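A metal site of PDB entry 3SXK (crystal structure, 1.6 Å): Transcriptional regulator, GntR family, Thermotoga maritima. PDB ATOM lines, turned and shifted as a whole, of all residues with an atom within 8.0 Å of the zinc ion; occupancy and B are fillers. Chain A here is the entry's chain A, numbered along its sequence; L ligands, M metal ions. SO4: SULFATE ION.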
ATOM      1  N   ARG A  15      -7.860   2.587   2.410  1.00  0.00           N
ATOM      2  CA  ARG A  15      -7.484   1.419   1.614  1.00  0.00           C
ATOM      3  C   ARG A  15      -6.257   0.739   2.192  1.00  0.00           C
ATOM      4  O   ARG A  15      -6.217  -0.499   2.265  1.00  0.00           O
ATOM      5  CB  ARG A  15      -7.198   1.817   0.167  1.00  0.00           C
ATOM      6  CG  ARG A  15      -8.438   2.284  -0.575  1.00  0.00           C
ATOM      7  CD  ARG A  15      -8.126   2.566  -2.045  1.00  0.00           C
ATOM      8  NE  ARG A  15      -7.802   1.365  -2.781  1.00  0.00           N
ATOM      9  CZ  ARG A  15      -7.366   1.340  -4.034  1.00  0.00           C
ATOM     10  NH1 ARG A  15      -7.273   2.458  -4.735  1.00  0.00           N
ATOM     11  NH2 ARG A  15      -7.054   0.186  -4.587  1.00  0.00           N
ATOM     12  N   GLU A  19      -6.805  -3.081   3.108  1.00  0.00           N
ATOM     13  CA  GLU A  19      -6.191  -4.009   2.171  1.00  0.00           C
ATOM     14  C   GLU A  19      -4.905  -4.615   2.752  1.00  0.00           C
ATOM     15  O   GLU A  19      -4.665  -5.785   2.583  1.00  0.00           O
ATOM     16  CB  GLU A  19      -5.854  -3.345   0.820  1.00  0.00           C
ATOM     17  CG  GLU A  19      -7.080  -2.814   0.062  1.00  0.00           C
ATOM     18  CD  GLU A  19      -6.732  -2.245  -1.288  1.00  0.00           C
ATOM     19  OE1 GLU A  19      -5.669  -2.708  -1.817  1.00  0.00           O
ATOM     20  OE2 GLU A  19      -7.512  -1.418  -1.871  1.00  0.00           O
ATOM     21  N   PHE A  55      -6.306  -2.658 -17.373  1.00  0.00           N
ATOM     22  CA  PHE A  55      -6.331  -2.037 -16.058  1.00  0.00           C
ATOM     23  C   PHE A  55      -7.644  -2.103 -15.253  1.00  0.00           C
ATOM     24  O   PHE A  55      -7.628  -2.652 -14.164  1.00  0.00           O
ATOM     25  CB  PHE A  55      -5.834  -0.602 -16.086  1.00  0.00           C
ATOM     26  CG  PHE A  55      -5.824   0.050 -14.714  1.00  0.00           C
ATOM     27  CD1 PHE A  55      -4.703  -0.049 -13.873  1.00  0.00           C
ATOM     28  CD2 PHE A  55      -6.932   0.732 -14.252  1.00  0.00           C
ATOM     29  CE1 PHE A  55      -4.724   0.554 -12.608  1.00  0.00           C
ATOM     30  CE2 PHE A  55      -6.944   1.325 -12.976  1.00  0.00           C
ATOM     31  CZ  PHE A  55      -5.832   1.232 -12.170  1.00  0.00           C
ATOM     32  N   SER A  58      -8.660  -5.672 -14.166  1.00  0.00           N
ATOM     33  CA  SER A  58      -7.665  -6.353 -13.308  1.00  0.00           C
ATOM     34  C   SER A  58      -7.478  -5.618 -11.978  1.00  0.00           C
ATOM     35  O   SER A  58      -7.266  -6.268 -10.950  1.00  0.00           O
ATOM     36  CB  SER A  58      -6.282  -6.561 -13.969  1.00  0.00           C
ATOM     37  OG  SER A  58      -5.661  -5.327 -14.277  1.00  0.00           O
ATOM     38  N   ASP A  59      -7.531  -4.293 -11.989  1.00  0.00           N
ATOM     39  CA  ASP A  59      -7.265  -3.493 -10.799  1.00  0.00           C
ATOM     40  C   ASP A  59      -8.328  -3.733  -9.704  1.00  0.00           C
ATOM     41  O   ASP A  59      -7.996  -4.078  -8.554  1.00  0.00           O
ATOM     42  CB  ASP A  59      -7.221  -2.002 -11.152  1.00  0.00           C
ATOM     43  CG  ASP A  59      -7.035  -1.133  -9.918  1.00  0.00           C
ATOM     44  OD1 ASP A  59      -5.984  -1.281  -9.277  1.00  0.00           O
ATOM     45  OD2 ASP A  59      -7.963  -0.357  -9.538  1.00  0.00           O
ATOM     46  N   GLU A  60      -9.602  -3.614 -10.073  1.00  0.00           N
ATOM     47  CA  GLU A  60     -10.690  -3.845  -9.130  1.00  0.00           C
ATOM     48  C   GLU A  60     -10.601  -5.265  -8.581  1.00  0.00           C
ATOM     49  O   GLU A  60     -10.704  -5.490  -7.343  1.00  0.00           O
ATOM     50  CB  GLU A  60     -12.041  -3.623  -9.789  1.00  0.00           C
ATOM     51  CG  GLU A  60     -13.194  -3.940  -8.855  1.00  0.00           C
ATOM     52  CD  GLU A  60     -14.548  -3.497  -9.320  1.00  0.00           C
ATOM     53  OE1 GLU A  60     -14.667  -2.945 -10.432  1.00  0.00           O
ATOM     54  OE2 GLU A  60     -15.497  -3.691  -8.540  1.00  0.00           O
ATOM     55  N   LEU A  62      -8.026  -7.315  -8.306  1.00  0.00           N
ATOM     56  CA  LEU A  62      -6.863  -7.578  -7.446  1.00  0.00           C
ATOM     57  C   LEU A  62      -7.069  -7.010  -6.045  1.00  0.00           C
ATOM     58  O   LEU A  62      -6.886  -7.741  -5.035  1.00  0.00           O
ATOM     59  CB  LEU A  62      -5.600  -6.994  -8.084  1.00  0.00           C
ATOM     60  CG  LEU A  62      -4.311  -7.196  -7.293  1.00  0.00           C
ATOM     61  CD1 LEU A  62      -3.992  -8.669  -7.067  1.00  0.00           C
ATOM     62  CD2 LEU A  62      -3.127  -6.536  -7.996  1.00  0.00           C
ATOM     63  N   HIS A  63      -7.454  -5.739  -5.954  1.00  0.00           N
ATOM     64  CA  HIS A  63      -7.690  -5.106  -4.673  1.00  0.00           C
ATOM     65  C   HIS A  63      -8.862  -5.752  -3.927  1.00  0.00           C
ATOM     66  O   HIS A  63      -8.796  -5.941  -2.685  1.00  0.00           O
ATOM     67  CB  HIS A  63      -7.853  -3.598  -4.866  1.00  0.00           C
ATOM     68  CG  HIS A  63      -6.582  -2.908  -5.270  1.00  0.00           C
ATOM     69  ND1 HIS A  63      -5.602  -2.557  -4.375  1.00  0.00           N
ATOM     70  CD2 HIS A  63      -6.161  -2.468  -6.486  1.00  0.00           C
ATOM     71  CE1 HIS A  63      -4.605  -1.965  -5.023  1.00  0.00           C
ATOM     72  NE2 HIS A  63      -4.937  -1.873  -6.291  1.00  0.00           N
ATOM     73  N   PHE A  66      -7.979  -9.185  -2.149  1.00  0.00           N
ATOM     74  CA  PHE A  66      -7.306  -9.139  -0.869  1.00  0.00           C
ATOM     75  C   PHE A  66      -8.379  -9.125   0.240  1.00  0.00           C
ATOM     76  O   PHE A  66      -8.271  -9.834   1.232  1.00  0.00           O
ATOM     77  CB  PHE A  66      -6.402  -7.937  -0.756  1.00  0.00           C
ATOM     78  CG  PHE A  66      -5.273  -7.884  -1.798  1.00  0.00           C
ATOM     79  CD1 PHE A  66      -4.773  -9.024  -2.406  1.00  0.00           C
ATOM     80  CD2 PHE A  66      -4.808  -6.657  -2.207  1.00  0.00           C
ATOM     81  CE1 PHE A  66      -3.758  -8.898  -3.380  1.00  0.00           C
ATOM     82  CE2 PHE A  66      -3.811  -6.538  -3.134  1.00  0.00           C
ATOM     83  CZ  PHE A  66      -3.294  -7.669  -3.711  1.00  0.00           C
ATOM     84  N   ARG A  90      -9.585   6.637  -8.078  1.00  0.00           N
ATOM     85  CA  ARG A  90      -8.711   6.033  -9.073  1.00  0.00           C
ATOM     86  C   ARG A  90      -8.862   6.685 -10.450  1.00  0.00           C
ATOM     87  O   ARG A  90      -7.889   6.724 -11.225  1.00  0.00           O
ATOM     88  CB  ARG A  90      -8.838   4.523  -9.137  1.00  0.00           C
ATOM     89  CG  ARG A  90     -10.034   3.988  -9.738  1.00  0.00           C
ATOM     90  CD  ARG A  90     -10.035   2.416  -9.648  1.00  0.00           C
ATOM     91  NE  ARG A  90     -11.250   1.952 -10.295  1.00  0.00           N
ATOM     92  CZ  ARG A  90     -11.422   0.793 -10.938  1.00  0.00           C
ATOM     93  NH1 ARG A  90     -10.474  -0.118 -10.981  1.00  0.00           N
ATOM     94  NH2 ARG A  90     -12.588   0.500 -11.460  1.00  0.00           N
ATOM     95  N   ARG A  95      -3.031   6.310 -14.579  1.00  0.00           N
ATOM     96  CA  ARG A  95      -1.687   5.744 -14.411  1.00  0.00           C
ATOM     97  C   ARG A  95      -1.581   4.309 -14.873  1.00  0.00           C
ATOM     98  O   ARG A  95      -0.840   3.499 -14.285  1.00  0.00           O
ATOM     99  CB  ARG A  95      -1.370   5.872 -12.918  1.00  0.00           C
ATOM    100  CG  ARG A  95       0.063   5.812 -12.563  1.00  0.00           C
ATOM    101  CD  ARG A  95       0.218   6.246 -11.122  1.00  0.00           C
ATOM    102  NE  ARG A  95       1.573   6.079 -10.632  1.00  0.00           N
ATOM    103  CZ  ARG A  95       1.984   4.984  -9.973  1.00  0.00           C
ATOM    104  NH1 ARG A  95       1.171   3.944  -9.792  1.00  0.00           N
ATOM    105  NH2 ARG A  95       3.240   4.936  -9.527  1.00  0.00           N
ATOM    106  N   SER A  99       0.774   1.710 -12.860  1.00  0.00           N
ATOM    107  CA  SER A  99       0.063   0.938 -11.846  1.00  0.00           C
ATOM    108  C   SER A  99      -0.013  -0.538 -12.228  1.00  0.00           C
ATOM    109  O   SER A  99       0.102  -1.419 -11.366  1.00  0.00           O
ATOM    110  CB  SER A  99      -1.337   1.489 -11.567  1.00  0.00           C
ATOM    111  OG  SER A  99      -1.257   2.691 -10.838  1.00  0.00           O
ATOM    112  N   ASN A 100      -0.133  -0.836 -13.516  1.00  0.00           N
ATOM    113  CA  ASN A 100      -0.150  -2.217 -13.931  1.00  0.00           C
ATOM    114  C   ASN A 100       1.205  -2.922 -13.633  1.00  0.00           C
ATOM    115  O   ASN A 100       1.227  -4.097 -13.194  1.00  0.00           O
ATOM    116  CB  ASN A 100      -0.525  -2.259 -15.412  1.00  0.00           C
ATOM    117  CG  ASN A 100      -0.640  -3.661 -15.925  1.00  0.00           C
ATOM    118  OD1 ASN A 100      -1.500  -4.421 -15.452  1.00  0.00           O
ATOM    119  ND2 ASN A 100       0.187  -4.014 -16.898  1.00  0.00           N
ATOM    120  N   GLU A 102       3.174  -2.136 -11.191  1.00  0.00           N
ATOM    121  CA  GLU A 102       3.198  -2.321  -9.726  1.00  0.00           C
ATOM    122  C   GLU A 102       2.334  -3.496  -9.299  1.00  0.00           C
ATOM    123  O   GLU A 102       2.706  -4.257  -8.427  1.00  0.00           O
ATOM    124  CB  GLU A 102       2.779  -1.035  -9.024  1.00  0.00           C
ATOM    125  CG  GLU A 102       3.834   0.082  -9.139  1.00  0.00           C
ATOM    126  CD  GLU A 102       3.377   1.475  -8.690  1.00  0.00           C
ATOM    127  OE1 GLU A 102       2.185   1.672  -8.362  1.00  0.00           O
ATOM    128  OE2 GLU A 102       4.214   2.418  -8.721  1.00  0.00           O
ATOM    129  N   HIS A 103       1.192  -3.680  -9.962  1.00  0.00           N
ATOM    130  CA  HIS A 103       0.341  -4.840  -9.704  1.00  0.00           C
ATOM    131  C   HIS A 103       1.094  -6.124 -10.044  1.00  0.00           C
ATOM    132  O   HIS A 103       1.040  -7.122  -9.294  1.00  0.00           O
ATOM    133  CB  HIS A 103      -0.924  -4.779 -10.551  1.00  0.00           C
ATOM    134  CG  HIS A 103      -1.858  -3.694 -10.146  1.00  0.00           C
ATOM    135  ND1 HIS A 103      -2.838  -3.196 -10.990  1.00  0.00           N
ATOM    136  CD2 HIS A 103      -1.975  -3.023  -8.979  1.00  0.00           C
ATOM    137  CE1 HIS A 103      -3.519  -2.261 -10.341  1.00  0.00           C
ATOM    138  NE2 HIS A 103      -3.003  -2.132  -9.129  1.00  0.00           N
ATOM    139  N   LEU A 106       3.652  -6.867  -7.428  1.00  0.00           N
ATOM    140  CA  LEU A 106       2.982  -7.231  -6.167  1.00  0.00           C
ATOM    141  C   LEU A 106       2.571  -8.695  -6.244  1.00  0.00           C
ATOM    142  O   LEU A 106       2.805  -9.490  -5.342  1.00  0.00           O
ATOM    143  CB  LEU A 106       1.757  -6.294  -5.963  1.00  0.00           C
ATOM    144  CG  LEU A 106       0.814  -6.687  -4.829  1.00  0.00           C
ATOM    145  CD1 LEU A 106       1.532  -6.941  -3.512  1.00  0.00           C
ATOM    146  CD2 LEU A 106      -0.295  -5.639  -4.644  1.00  0.00           C
ATOM    147  N   LEU A 122       2.484  -3.355  -1.673  1.00  0.00           N
ATOM    148  CA  LEU A 122       1.106  -2.855  -1.675  1.00  0.00           C
ATOM    149  C   LEU A 122       1.093  -1.435  -1.109  1.00  0.00           C
ATOM    150  O   LEU A 122       0.435  -0.557  -1.642  1.00  0.00           O
ATOM    151  CB  LEU A 122       0.138  -3.800  -0.927  1.00  0.00           C
ATOM    152  CG  LEU A 122      -1.299  -3.276  -0.806  1.00  0.00           C
ATOM    153  CD1 LEU A 122      -1.882  -2.937  -2.145  1.00  0.00           C
ATOM    154  CD2 LEU A 122      -2.105  -4.361  -0.100  1.00  0.00           C
ATOM    155  N   HIS A 125       2.767   0.916  -3.643  1.00  0.00           N
ATOM    156  CA  HIS A 125       1.813   1.119  -4.746  1.00  0.00           C
ATOM    157  C   HIS A 125       0.718   2.153  -4.405  1.00  0.00           C
ATOM    158  O   HIS A 125       0.483   3.093  -5.151  1.00  0.00           O
ATOM    159  CB  HIS A 125       1.207  -0.244  -5.099  1.00  0.00           C
ATOM    160  CG  HIS A 125       0.009  -0.191  -5.994  1.00  0.00           C
ATOM    161  ND1 HIS A 125       0.005   0.433  -7.230  1.00  0.00           N
ATOM    162  CD2 HIS A 125      -1.248  -0.647  -5.800  1.00  0.00           C
ATOM    163  CE1 HIS A 125      -1.199   0.307  -7.780  1.00  0.00           C
ATOM    164  NE2 HIS A 125      -1.984  -0.311  -6.913  1.00  0.00           N
ATOM    165  N   LEU A 126       0.013   1.955  -3.284  1.00  0.00           N
ATOM    166  CA  LEU A 126      -1.039   2.887  -2.910  1.00  0.00           C
ATOM    167  C   LEU A 126      -0.490   4.280  -2.622  1.00  0.00           C
ATOM    168  O   LEU A 126      -1.094   5.252  -3.023  1.00  0.00           O
ATOM    169  CB  LEU A 126      -1.856   2.352  -1.731  1.00  0.00           C
ATOM    170  CG  LEU A 126      -2.721   1.125  -2.075  1.00  0.00           C
ATOM    171  CD1 LEU A 126      -3.288   0.427  -0.816  1.00  0.00           C
ATOM    172  CD2 LEU A 126      -3.832   1.475  -3.076  1.00  0.00           C
ATOM    173  N   VAL A 129       0.369   5.933  -5.958  1.00  0.00           N
ATOM    174  CA  VAL A 129      -0.844   6.366  -6.613  1.00  0.00           C
ATOM    175  C   VAL A 129      -1.338   7.664  -5.977  1.00  0.00           C
ATOM    176  O   VAL A 129      -1.712   8.600  -6.683  1.00  0.00           O
ATOM    177  CB  VAL A 129      -1.933   5.260  -6.506  1.00  0.00           C
ATOM    178  CG1 VAL A 129      -3.320   5.814  -6.850  1.00  0.00           C
ATOM    179  CG2 VAL A 129      -1.583   4.073  -7.385  1.00  0.00           C
HETATM  180  S   SO4 L   1      -5.513   1.809  -7.858  1.00  0.00           S
HETATM  181  O1  SO4 L   1      -6.766   1.013  -7.566  1.00  0.00           O
HETATM  182  O2  SO4 L   1      -5.096   2.605  -6.707  1.00  0.00           O
HETATM  183  O3  SO4 L   1      -4.397   0.943  -8.443  1.00  0.00           O
HETATM  184  O4  SO4 L   1      -5.730   2.863  -8.813  1.00  0.00           O
HETATM  185 ZN    ZN M   1      -3.841  -0.916  -7.754  1.00  0.00          ZN
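Within 4 Å of the zinc ion: Asp 59, His 63, His 103 and His 125.
The nearest printed residue that does not touch the zinc ion is Arg 15 (4.6 Å).
A ring nitrogen (NE2) of His 103 lies close to the side-chain carboxylate of Asp 59.
A ring nitrogen (ND1) of His 63 lies within hydrogen-bond range of the guanidinium group (NH2) of Arg 15, at 3.1 Å.
OE1 of Glu 19 sits at hydrogen-bond distance from ND1 of His 63.
A ring nitrogen (ND1) of His 103 lies close to the backbone carbonyl oxygen of Ser 99, 3.5 Å away.
NE2 of His 63 sits close to OD1 of Asp 59 (3.2 Å).
The side-chain carboxylate (OE1) of Glu 102 is in hydrogen-bond range of a ring nitrogen (ND1) of His 125, at 2.8 Å.
OD2 of Asp 59 lies within salt-bridge range of NH1 of Arg 90, 2.9 Å away.
NE2 of His 103 binds the zinc ion.
O3 of the ligand is bound to the zinc ion, 2.1 Å away.
The zinc ion is bound by NE2 of His 63 (2.1 Å).
A ring nitrogen (NE2) of His 125 binds the zinc ion, 2.1 Å away.
Slightly farther from the zinc ion lies OD1 of Asp 59 (2.7 Å).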
